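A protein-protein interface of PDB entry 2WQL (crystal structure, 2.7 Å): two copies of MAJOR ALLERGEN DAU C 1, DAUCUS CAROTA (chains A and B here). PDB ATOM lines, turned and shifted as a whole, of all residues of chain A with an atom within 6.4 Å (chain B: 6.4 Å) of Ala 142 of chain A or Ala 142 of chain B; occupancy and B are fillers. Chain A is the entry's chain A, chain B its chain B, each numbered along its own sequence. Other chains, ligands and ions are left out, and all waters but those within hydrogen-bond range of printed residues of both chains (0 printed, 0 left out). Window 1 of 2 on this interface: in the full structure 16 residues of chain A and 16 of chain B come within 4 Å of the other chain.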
ATOM      1  N   ASP A 137      -8.512 -21.865   5.316  1.00  0.00           N
ATOM      2  CA  ASP A 137      -9.358 -22.637   6.245  1.00  0.00           C
ATOM      3  C   ASP A 137     -10.850 -22.553   5.917  1.00  0.00           C
ATOM      4  O   ASP A 137     -11.568 -23.555   5.963  1.00  0.00           O
ATOM      5  CB  ASP A 137      -9.149 -22.162   7.686  1.00  0.00           C
ATOM      6  CG  ASP A 137      -7.824 -22.622   8.271  1.00  0.00           C
ATOM      7  OD1 ASP A 137      -7.116 -23.464   7.630  1.00  0.00           O
ATOM      8  OD2 ASP A 137      -7.502 -22.142   9.397  1.00  0.00           O
ATOM      9  N   ALA A 138     -11.305 -21.346   5.596  1.00  0.00           N
ATOM     10  CA  ALA A 138     -12.699 -21.122   5.248  1.00  0.00           C
ATOM     11  C   ALA A 138     -13.048 -21.901   3.992  1.00  0.00           C
ATOM     12  O   ALA A 138     -14.086 -22.563   3.932  1.00  0.00           O
ATOM     13  CB  ALA A 138     -12.968 -19.673   5.042  1.00  0.00           C
ATOM     14  N   GLN A 139     -12.169 -21.838   3.000  1.00  0.00           N
ATOM     15  CA  GLN A 139     -12.462 -22.410   1.705  1.00  0.00           C
ATOM     16  C   GLN A 139     -12.389 -23.941   1.753  1.00  0.00           C
ATOM     17  O   GLN A 139     -13.197 -24.632   1.120  1.00  0.00           O
ATOM     18  CB  GLN A 139     -11.511 -21.824   0.680  1.00  0.00           C
ATOM     19  CG  GLN A 139     -11.795 -22.230  -0.734  1.00  0.00           C
ATOM     20  CD  GLN A 139     -11.512 -21.113  -1.710  1.00  0.00           C
ATOM     21  OE1 GLN A 139     -12.335 -20.196  -1.861  1.00  0.00           O
ATOM     22  NE2 GLN A 139     -10.351 -21.187  -2.391  1.00  0.00           N
ATOM     23  N   ASN A 140     -11.436 -24.467   2.514  1.00  0.00           N
ATOM     24  CA  ASN A 140     -11.298 -25.908   2.668  1.00  0.00           C
ATOM     25  C   ASN A 140     -12.470 -26.489   3.455  1.00  0.00           C
ATOM     26  O   ASN A 140     -12.928 -27.599   3.181  1.00  0.00           O
ATOM     27  CB  ASN A 140      -9.963 -26.256   3.338  1.00  0.00           C
ATOM     28  CG  ASN A 140      -8.783 -26.160   2.373  1.00  0.00           C
ATOM     29  OD1 ASN A 140      -8.867 -26.566   1.221  1.00  0.00           O
ATOM     30  ND2 ASN A 140      -7.678 -25.593   2.841  1.00  0.00           N
ATOM     31  N   THR A 141     -12.947 -25.730   4.433  1.00  0.00           N
ATOM     32  CA  THR A 141     -14.102 -26.135   5.210  1.00  0.00           C
ATOM     33  C   THR A 141     -15.345 -26.117   4.324  1.00  0.00           C
ATOM     34  O   THR A 141     -16.136 -27.031   4.359  1.00  0.00           O
ATOM     35  CB  THR A 141     -14.284 -25.235   6.453  1.00  0.00           C
ATOM     36  OG1 THR A 141     -13.092 -25.269   7.235  1.00  0.00           O
ATOM     37  CG2 THR A 141     -15.451 -25.706   7.306  1.00  0.00           C
ATOM     38  N   ALA A 142     -15.492 -25.077   3.515  1.00  0.00           N
ATOM     39  CA  ALA A 142     -16.617 -24.967   2.577  1.00  0.00           C
ATOM     40  C   ALA A 142     -16.703 -26.196   1.675  1.00  0.00           C
ATOM     41  O   ALA A 142     -17.768 -26.768   1.481  1.00  0.00           O
ATOM     42  CB  ALA A 142     -16.497 -23.706   1.724  1.00  0.00           C
ATOM     43  N   LEU A 143     -15.566 -26.598   1.124  1.00  0.00           N
ATOM     44  CA  LEU A 143     -15.516 -27.734   0.235  1.00  0.00           C
ATOM     45  C   LEU A 143     -15.754 -29.038   1.009  1.00  0.00           C
ATOM     46  O   LEU A 143     -16.506 -29.905   0.554  1.00  0.00           O
ATOM     47  CB  LEU A 143     -14.176 -27.772  -0.502  1.00  0.00           C
ATOM     48  CG  LEU A 143     -14.020 -28.839  -1.588  1.00  0.00           C
ATOM     49  CD1 LEU A 143     -15.123 -28.695  -2.636  1.00  0.00           C
ATOM     50  CD2 LEU A 143     -12.621 -28.740  -2.211  1.00  0.00           C
ATOM     51  N   PHE A 144     -15.139 -29.166   2.176  1.00  0.00           N
ATOM     52  CA  PHE A 144     -15.371 -30.319   3.044  1.00  0.00           C
ATOM     53  C   PHE A 144     -16.863 -30.534   3.281  1.00  0.00           C
ATOM     54  O   PHE A 144     -17.373 -31.647   3.113  1.00  0.00           O
ATOM     55  CB  PHE A 144     -14.678 -30.122   4.395  1.00  0.00           C
ATOM     56  CG  PHE A 144     -14.840 -31.278   5.340  1.00  0.00           C
ATOM     57  CD1 PHE A 144     -13.829 -32.223   5.474  1.00  0.00           C
ATOM     58  CD2 PHE A 144     -15.979 -31.432   6.088  1.00  0.00           C
ATOM     59  CE1 PHE A 144     -13.956 -33.289   6.338  1.00  0.00           C
ATOM     60  CE2 PHE A 144     -16.120 -32.502   6.946  1.00  0.00           C
ATOM     61  CZ  PHE A 144     -15.095 -33.433   7.072  1.00  0.00           C
ATOM     62  N   LYS A 145     -17.553 -29.462   3.663  1.00  0.00           N
ATOM     63  CA  LYS A 145     -18.948 -29.543   4.042  1.00  0.00           C
ATOM     64  C   LYS A 145     -19.880 -29.761   2.856  1.00  0.00           C
ATOM     65  O   LYS A 145     -20.942 -30.363   2.994  1.00  0.00           O
ATOM     66  CB  LYS A 145     -19.354 -28.297   4.836  1.00  0.00           C
ATOM     67  CG  LYS A 145     -18.741 -28.221   6.250  1.00  0.00           C
ATOM     68  CD  LYS A 145     -19.207 -29.382   7.133  1.00  0.00           C
ATOM     69  CE  LYS A 145     -18.803 -29.236   8.604  1.00  0.00           C
ATOM     70  NZ  LYS A 145     -19.247 -30.450   9.395  1.00  0.00           N
ATOM     71  N   ALA A 146     -19.501 -29.270   1.686  1.00  0.00           N
ATOM     72  CA  ALA A 146     -20.270 -29.559   0.481  1.00  0.00           C
ATOM     73  C   ALA A 146     -20.202 -31.067   0.209  1.00  0.00           C
ATOM     74  O   ALA A 146     -21.192 -31.683  -0.172  1.00  0.00           O
ATOM     75  CB  ALA A 146     -19.742 -28.759  -0.708  1.00  0.00           C
ATOM     76  N   ILE A 147     -19.024 -31.653   0.424  1.00  0.00           N
ATOM     77  CA  ILE A 147     -18.826 -33.093   0.254  1.00  0.00           C
ATOM     78  C   ILE A 147     -19.577 -33.888   1.324  1.00  0.00           C
ATOM     79  O   ILE A 147     -20.220 -34.898   1.025  1.00  0.00           O
ATOM     80  CB  ILE A 147     -17.313 -33.466   0.241  1.00  0.00           C
ATOM     81  CG1 ILE A 147     -16.649 -32.960  -1.044  1.00  0.00           C
ATOM     82  CG2 ILE A 147     -17.103 -34.967   0.326  1.00  0.00           C
ATOM     83  CD1 ILE A 147     -15.139 -32.884  -0.965  1.00  0.00           C
ATOM     84  N   ALA A 149     -22.313 -33.032   2.703  1.00  0.00           N
ATOM     85  CA  ALA A 149     -23.702 -32.981   2.270  1.00  0.00           C
ATOM     86  C   ALA A 149     -23.996 -34.051   1.225  1.00  0.00           C
ATOM     87  O   ALA A 149     -25.016 -34.734   1.284  1.00  0.00           O
ATOM     88  CB  ALA A 149     -24.022 -31.616   1.729  1.00  0.00           C
ATOM     89  N   ASP B 137     -27.856 -28.877   7.332  1.00  0.00           N
ATOM     90  CA  ASP B 137     -26.780 -28.298   8.132  1.00  0.00           C
ATOM     91  C   ASP B 137     -25.451 -28.266   7.376  1.00  0.00           C
ATOM     92  O   ASP B 137     -24.721 -27.269   7.436  1.00  0.00           O
ATOM     93  CB  ASP B 137     -26.596 -29.087   9.428  1.00  0.00           C
ATOM     94  CG  ASP B 137     -27.717 -28.832  10.448  1.00  0.00           C
ATOM     95  OD1 ASP B 137     -28.570 -27.928  10.226  1.00  0.00           O
ATOM     96  OD2 ASP B 137     -27.748 -29.558  11.482  1.00  0.00           O
ATOM     97  N   ALA B 138     -25.138 -29.356   6.683  1.00  0.00           N
ATOM     98  CA  ALA B 138     -23.911 -29.434   5.916  1.00  0.00           C
ATOM     99  C   ALA B 138     -23.923 -28.376   4.824  1.00  0.00           C
ATOM    100  O   ALA B 138     -22.950 -27.653   4.641  1.00  0.00           O
ATOM    101  CB  ALA B 138     -23.733 -30.811   5.320  1.00  0.00           C
ATOM    102  N   GLN B 139     -25.034 -28.267   4.117  1.00  0.00           N
ATOM    103  CA  GLN B 139     -25.100 -27.410   2.960  1.00  0.00           C
ATOM    104  C   GLN B 139     -25.123 -25.926   3.343  1.00  0.00           C
ATOM    105  O   GLN B 139     -24.497 -25.105   2.684  1.00  0.00           O
ATOM    106  CB  GLN B 139     -26.320 -27.793   2.134  1.00  0.00           C
ATOM    107  CG  GLN B 139     -26.451 -27.054   0.803  1.00  0.00           C
ATOM    108  CD  GLN B 139     -27.034 -27.946  -0.276  1.00  0.00           C
ATOM    109  OE1 GLN B 139     -26.343 -28.845  -0.801  1.00  0.00           O
ATOM    110  NE2 GLN B 139     -28.312 -27.707  -0.617  1.00  0.00           N
ATOM    111  N   ASN B 140     -25.821 -25.600   4.427  1.00  0.00           N
ATOM    112  CA  ASN B 140     -25.838 -24.244   4.972  1.00  0.00           C
ATOM    113  C   ASN B 140     -24.475 -23.836   5.517  1.00  0.00           C
ATOM    114  O   ASN B 140     -24.078 -22.682   5.401  1.00  0.00           O
ATOM    115  CB  ASN B 140     -26.885 -24.120   6.085  1.00  0.00           C
ATOM    116  CG  ASN B 140     -28.305 -24.015   5.555  1.00  0.00           C
ATOM    117  OD1 ASN B 140     -28.568 -23.305   4.573  1.00  0.00           O
ATOM    118  ND2 ASN B 140     -29.241 -24.717   6.215  1.00  0.00           N
ATOM    119  N   THR B 141     -23.765 -24.782   6.123  1.00  0.00           N
ATOM    120  CA  THR B 141     -22.420 -24.521   6.625  1.00  0.00           C
ATOM    121  C   THR B 141     -21.450 -24.322   5.458  1.00  0.00           C
ATOM    122  O   THR B 141     -20.605 -23.426   5.495  1.00  0.00           O
ATOM    123  CB  THR B 141     -21.916 -25.659   7.565  1.00  0.00           C
ATOM    124  OG1 THR B 141     -22.820 -25.812   8.671  1.00  0.00           O
ATOM    125  CG2 THR B 141     -20.536 -25.339   8.129  1.00  0.00           C
ATOM    126  N   ALA B 142     -21.593 -25.140   4.420  1.00  0.00           N
ATOM    127  CA  ALA B 142     -20.794 -24.999   3.197  1.00  0.00           C
ATOM    128  C   ALA B 142     -20.929 -23.606   2.607  1.00  0.00           C
ATOM    129  O   ALA B 142     -19.932 -22.963   2.306  1.00  0.00           O
ATOM    130  CB  ALA B 142     -21.200 -26.046   2.168  1.00  0.00           C
ATOM    131  N   LEU B 143     -22.164 -23.137   2.477  1.00  0.00           N
ATOM    132  CA  LEU B 143     -22.426 -21.802   1.935  1.00  0.00           C
ATOM    133  C   LEU B 143     -21.922 -20.687   2.870  1.00  0.00           C
ATOM    134  O   LEU B 143     -21.315 -19.727   2.430  1.00  0.00           O
ATOM    135  CB  LEU B 143     -23.927 -21.632   1.645  1.00  0.00           C
ATOM    136  CG  LEU B 143     -24.330 -20.364   0.887  1.00  0.00           C
ATOM    137  CD1 LEU B 143     -23.543 -20.210  -0.420  1.00  0.00           C
ATOM    138  CD2 LEU B 143     -25.858 -20.380   0.638  1.00  0.00           C
ATOM    139  N   PHE B 144     -22.163 -20.842   4.163  1.00  0.00           N
ATOM    140  CA  PHE B 144     -21.656 -19.899   5.154  1.00  0.00           C
ATOM    141  C   PHE B 144     -20.158 -19.723   4.977  1.00  0.00           C
ATOM    142  O   PHE B 144     -19.661 -18.613   4.897  1.00  0.00           O
ATOM    143  CB  PHE B 144     -21.969 -20.397   6.565  1.00  0.00           C
ATOM    144  CG  PHE B 144     -21.520 -19.467   7.661  1.00  0.00           C
ATOM    145  CD1 PHE B 144     -22.424 -18.628   8.289  1.00  0.00           C
ATOM    146  CD2 PHE B 144     -20.200 -19.446   8.076  1.00  0.00           C
ATOM    147  CE1 PHE B 144     -22.026 -17.781   9.310  1.00  0.00           C
ATOM    148  CE2 PHE B 144     -19.794 -18.599   9.077  1.00  0.00           C
ATOM    149  CZ  PHE B 144     -20.713 -17.764   9.699  1.00  0.00           C
ATOM    150  N   LYS B 145     -19.442 -20.830   4.908  1.00  0.00           N
ATOM    151  CA  LYS B 145     -17.980 -20.780   4.900  1.00  0.00           C
ATOM    152  C   LYS B 145     -17.417 -20.258   3.593  1.00  0.00           C
ATOM    153  O   LYS B 145     -16.364 -19.654   3.576  1.00  0.00           O
ATOM    154  CB  LYS B 145     -17.387 -22.154   5.242  1.00  0.00           C
ATOM    155  CG  LYS B 145     -17.579 -22.561   6.720  1.00  0.00           C
ATOM    156  CD  LYS B 145     -16.865 -21.591   7.679  1.00  0.00           C
ATOM    157  CE  LYS B 145     -16.859 -22.067   9.137  1.00  0.00           C
ATOM    158  NZ  LYS B 145     -16.240 -21.045  10.063  1.00  0.00           N
ATOM    159  N   ALA B 146     -18.131 -20.482   2.495  1.00  0.00           N
ATOM    160  CA  ALA B 146     -17.748 -19.907   1.221  1.00  0.00           C
ATOM    161  C   ALA B 146     -17.820 -18.391   1.329  1.00  0.00           C
ATOM    162  O   ALA B 146     -16.921 -17.691   0.848  1.00  0.00           O
ATOM    163  CB  ALA B 146     -18.631 -20.423   0.115  1.00  0.00           C
ATOM    164  N   ILE B 147     -18.876 -17.900   1.977  1.00  0.00           N
ATOM    165  CA  ILE B 147     -19.077 -16.463   2.210  1.00  0.00           C
ATOM    166  C   ILE B 147     -18.045 -15.889   3.195  1.00  0.00           C
ATOM    167  O   ILE B 147     -17.494 -14.803   2.977  1.00  0.00           O
ATOM    168  CB  ILE B 147     -20.501 -16.165   2.715  1.00  0.00           C
ATOM    169  CG1 ILE B 147     -21.511 -16.377   1.580  1.00  0.00           C
ATOM    170  CG2 ILE B 147     -20.597 -14.750   3.217  1.00  0.00           C
ATOM    171  CD1 ILE B 147     -22.954 -16.488   2.016  1.00  0.00           C
ATOM    172  N   ALA B 149     -15.048 -16.955   3.515  1.00  0.00           N
ATOM    173  CA  ALA B 149     -13.840 -16.847   2.702  1.00  0.00           C
ATOM    174  C   ALA B 149     -13.819 -15.555   1.870  1.00  0.00           C
ATOM    175  O   ALA B 149     -12.799 -14.876   1.773  1.00  0.00           O
ATOM    176  CB  ALA B 149     -13.718 -18.056   1.797  1.00  0.00           C
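Ala 138 of chain A touches Ala 149 of chain B, and with the chains exchanged Ala 149 of chain A touches Ala 138 of chain B.
Thr 141 of chain A touches Lys 145 of chain B, and with the chains exchanged Lys 145 of chain A touches Thr 141 of chain B.
Ala 142 of chain A touches its own counterpart, Ala 142 of chain B.
Ala 142 of chain A touches Ala 146 of chain B, and with the chains exchanged Ala 146 of chain A touches Ala 142 of chain B.
Positions printed for both chains: 137, 138, 139, 140, 141, 142, 143, 144, 145, 146, 147 and 149.
Of the 12 printed residues of chain B, 6 touch a printed residue of chain A.
Hydrophobic or aromatic side chains of chain B within 4 Å of the printed part of chain A: Ala 138, Ala 142 and Ala 149.
Of the 12 printed residues of chain A, 6 touch a printed residue of chain B.
Hydrophobic or aromatic side chains of chain A within 4 Å of the printed part of chain B: Ala 138, Ala 142 and Ala 149.
Among the printed residues, 11 pairs touch across the chains.
Ala 142 of chain A touches just these residues of chain B: Ala 142, Lys 145 and Ala 146.
Of chain A, only Ala 142 (3.6 Å), Lys 145 (3.9 Å) and Ala 146 (3.7 Å) come within 4 Å of Ala 142 of chain B.
Of the printed residues of chain B, Lys 145 of chain A touches Ala 138, Thr 141 and Ala 142.
Of the printed residues of chain B, Ala 149 of chain A touches Ala 138.
Of the printed residues of chain A, Lys 145 of chain B touches Ala 138, Thr 141 and Ala 142.
Of the printed residues of chain B, Ala 138 of chain A touches Lys 145 (3.6 Å) and Ala 149 (3.7 Å).
Printed residues of chain A within 4 Å of Ala 146 of chain B: Ala 142.
Leu 143 of chain A touches none of the printed residues of chain B.
The nearest residue of chain A that does not touch Ala 142 of chain B is Thr 141 of chain A (5.2 Å).
Ala 138 of chain A touches Lys 145 of chain B.
Ala 138 of chain A touches Ala 149 of chain B (CB to CB, 3.7 Å).
Thr 141 of chain A touches Lys 145 of chain B.
Ala 142 of chain B touches Ala 142 of chain A (O to CB, 3.6 Å).
CB of Lys 145 of chain B touches N of Ala 142 of chain A, 3.9 Å away.
CB of Ala 142 of chain A touches N of Ala 146 of chain B (3.7 Å).
O of Ala 138 of chain B touches CB of Lys 145 of chain A, at 3.7 Å.
N of Ala 142 of chain B touches CB of Lys 145 of chain A, 3.9 Å away.
Ala 142 of chain B touches Ala 146 of chain A.
Ala 149 of chain A touches Ala 138 of chain B.
OG1 of Thr 141 of chain A lies within hydrogen-bond range of O of Asp 137 of chain A (2.6 Å).
The backbone carbonyl oxygen (O) of Asp 137 of chain B lies within hydrogen-bond range of the side-chain hydroxyl (OG1) of Thr 141 of chain B.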
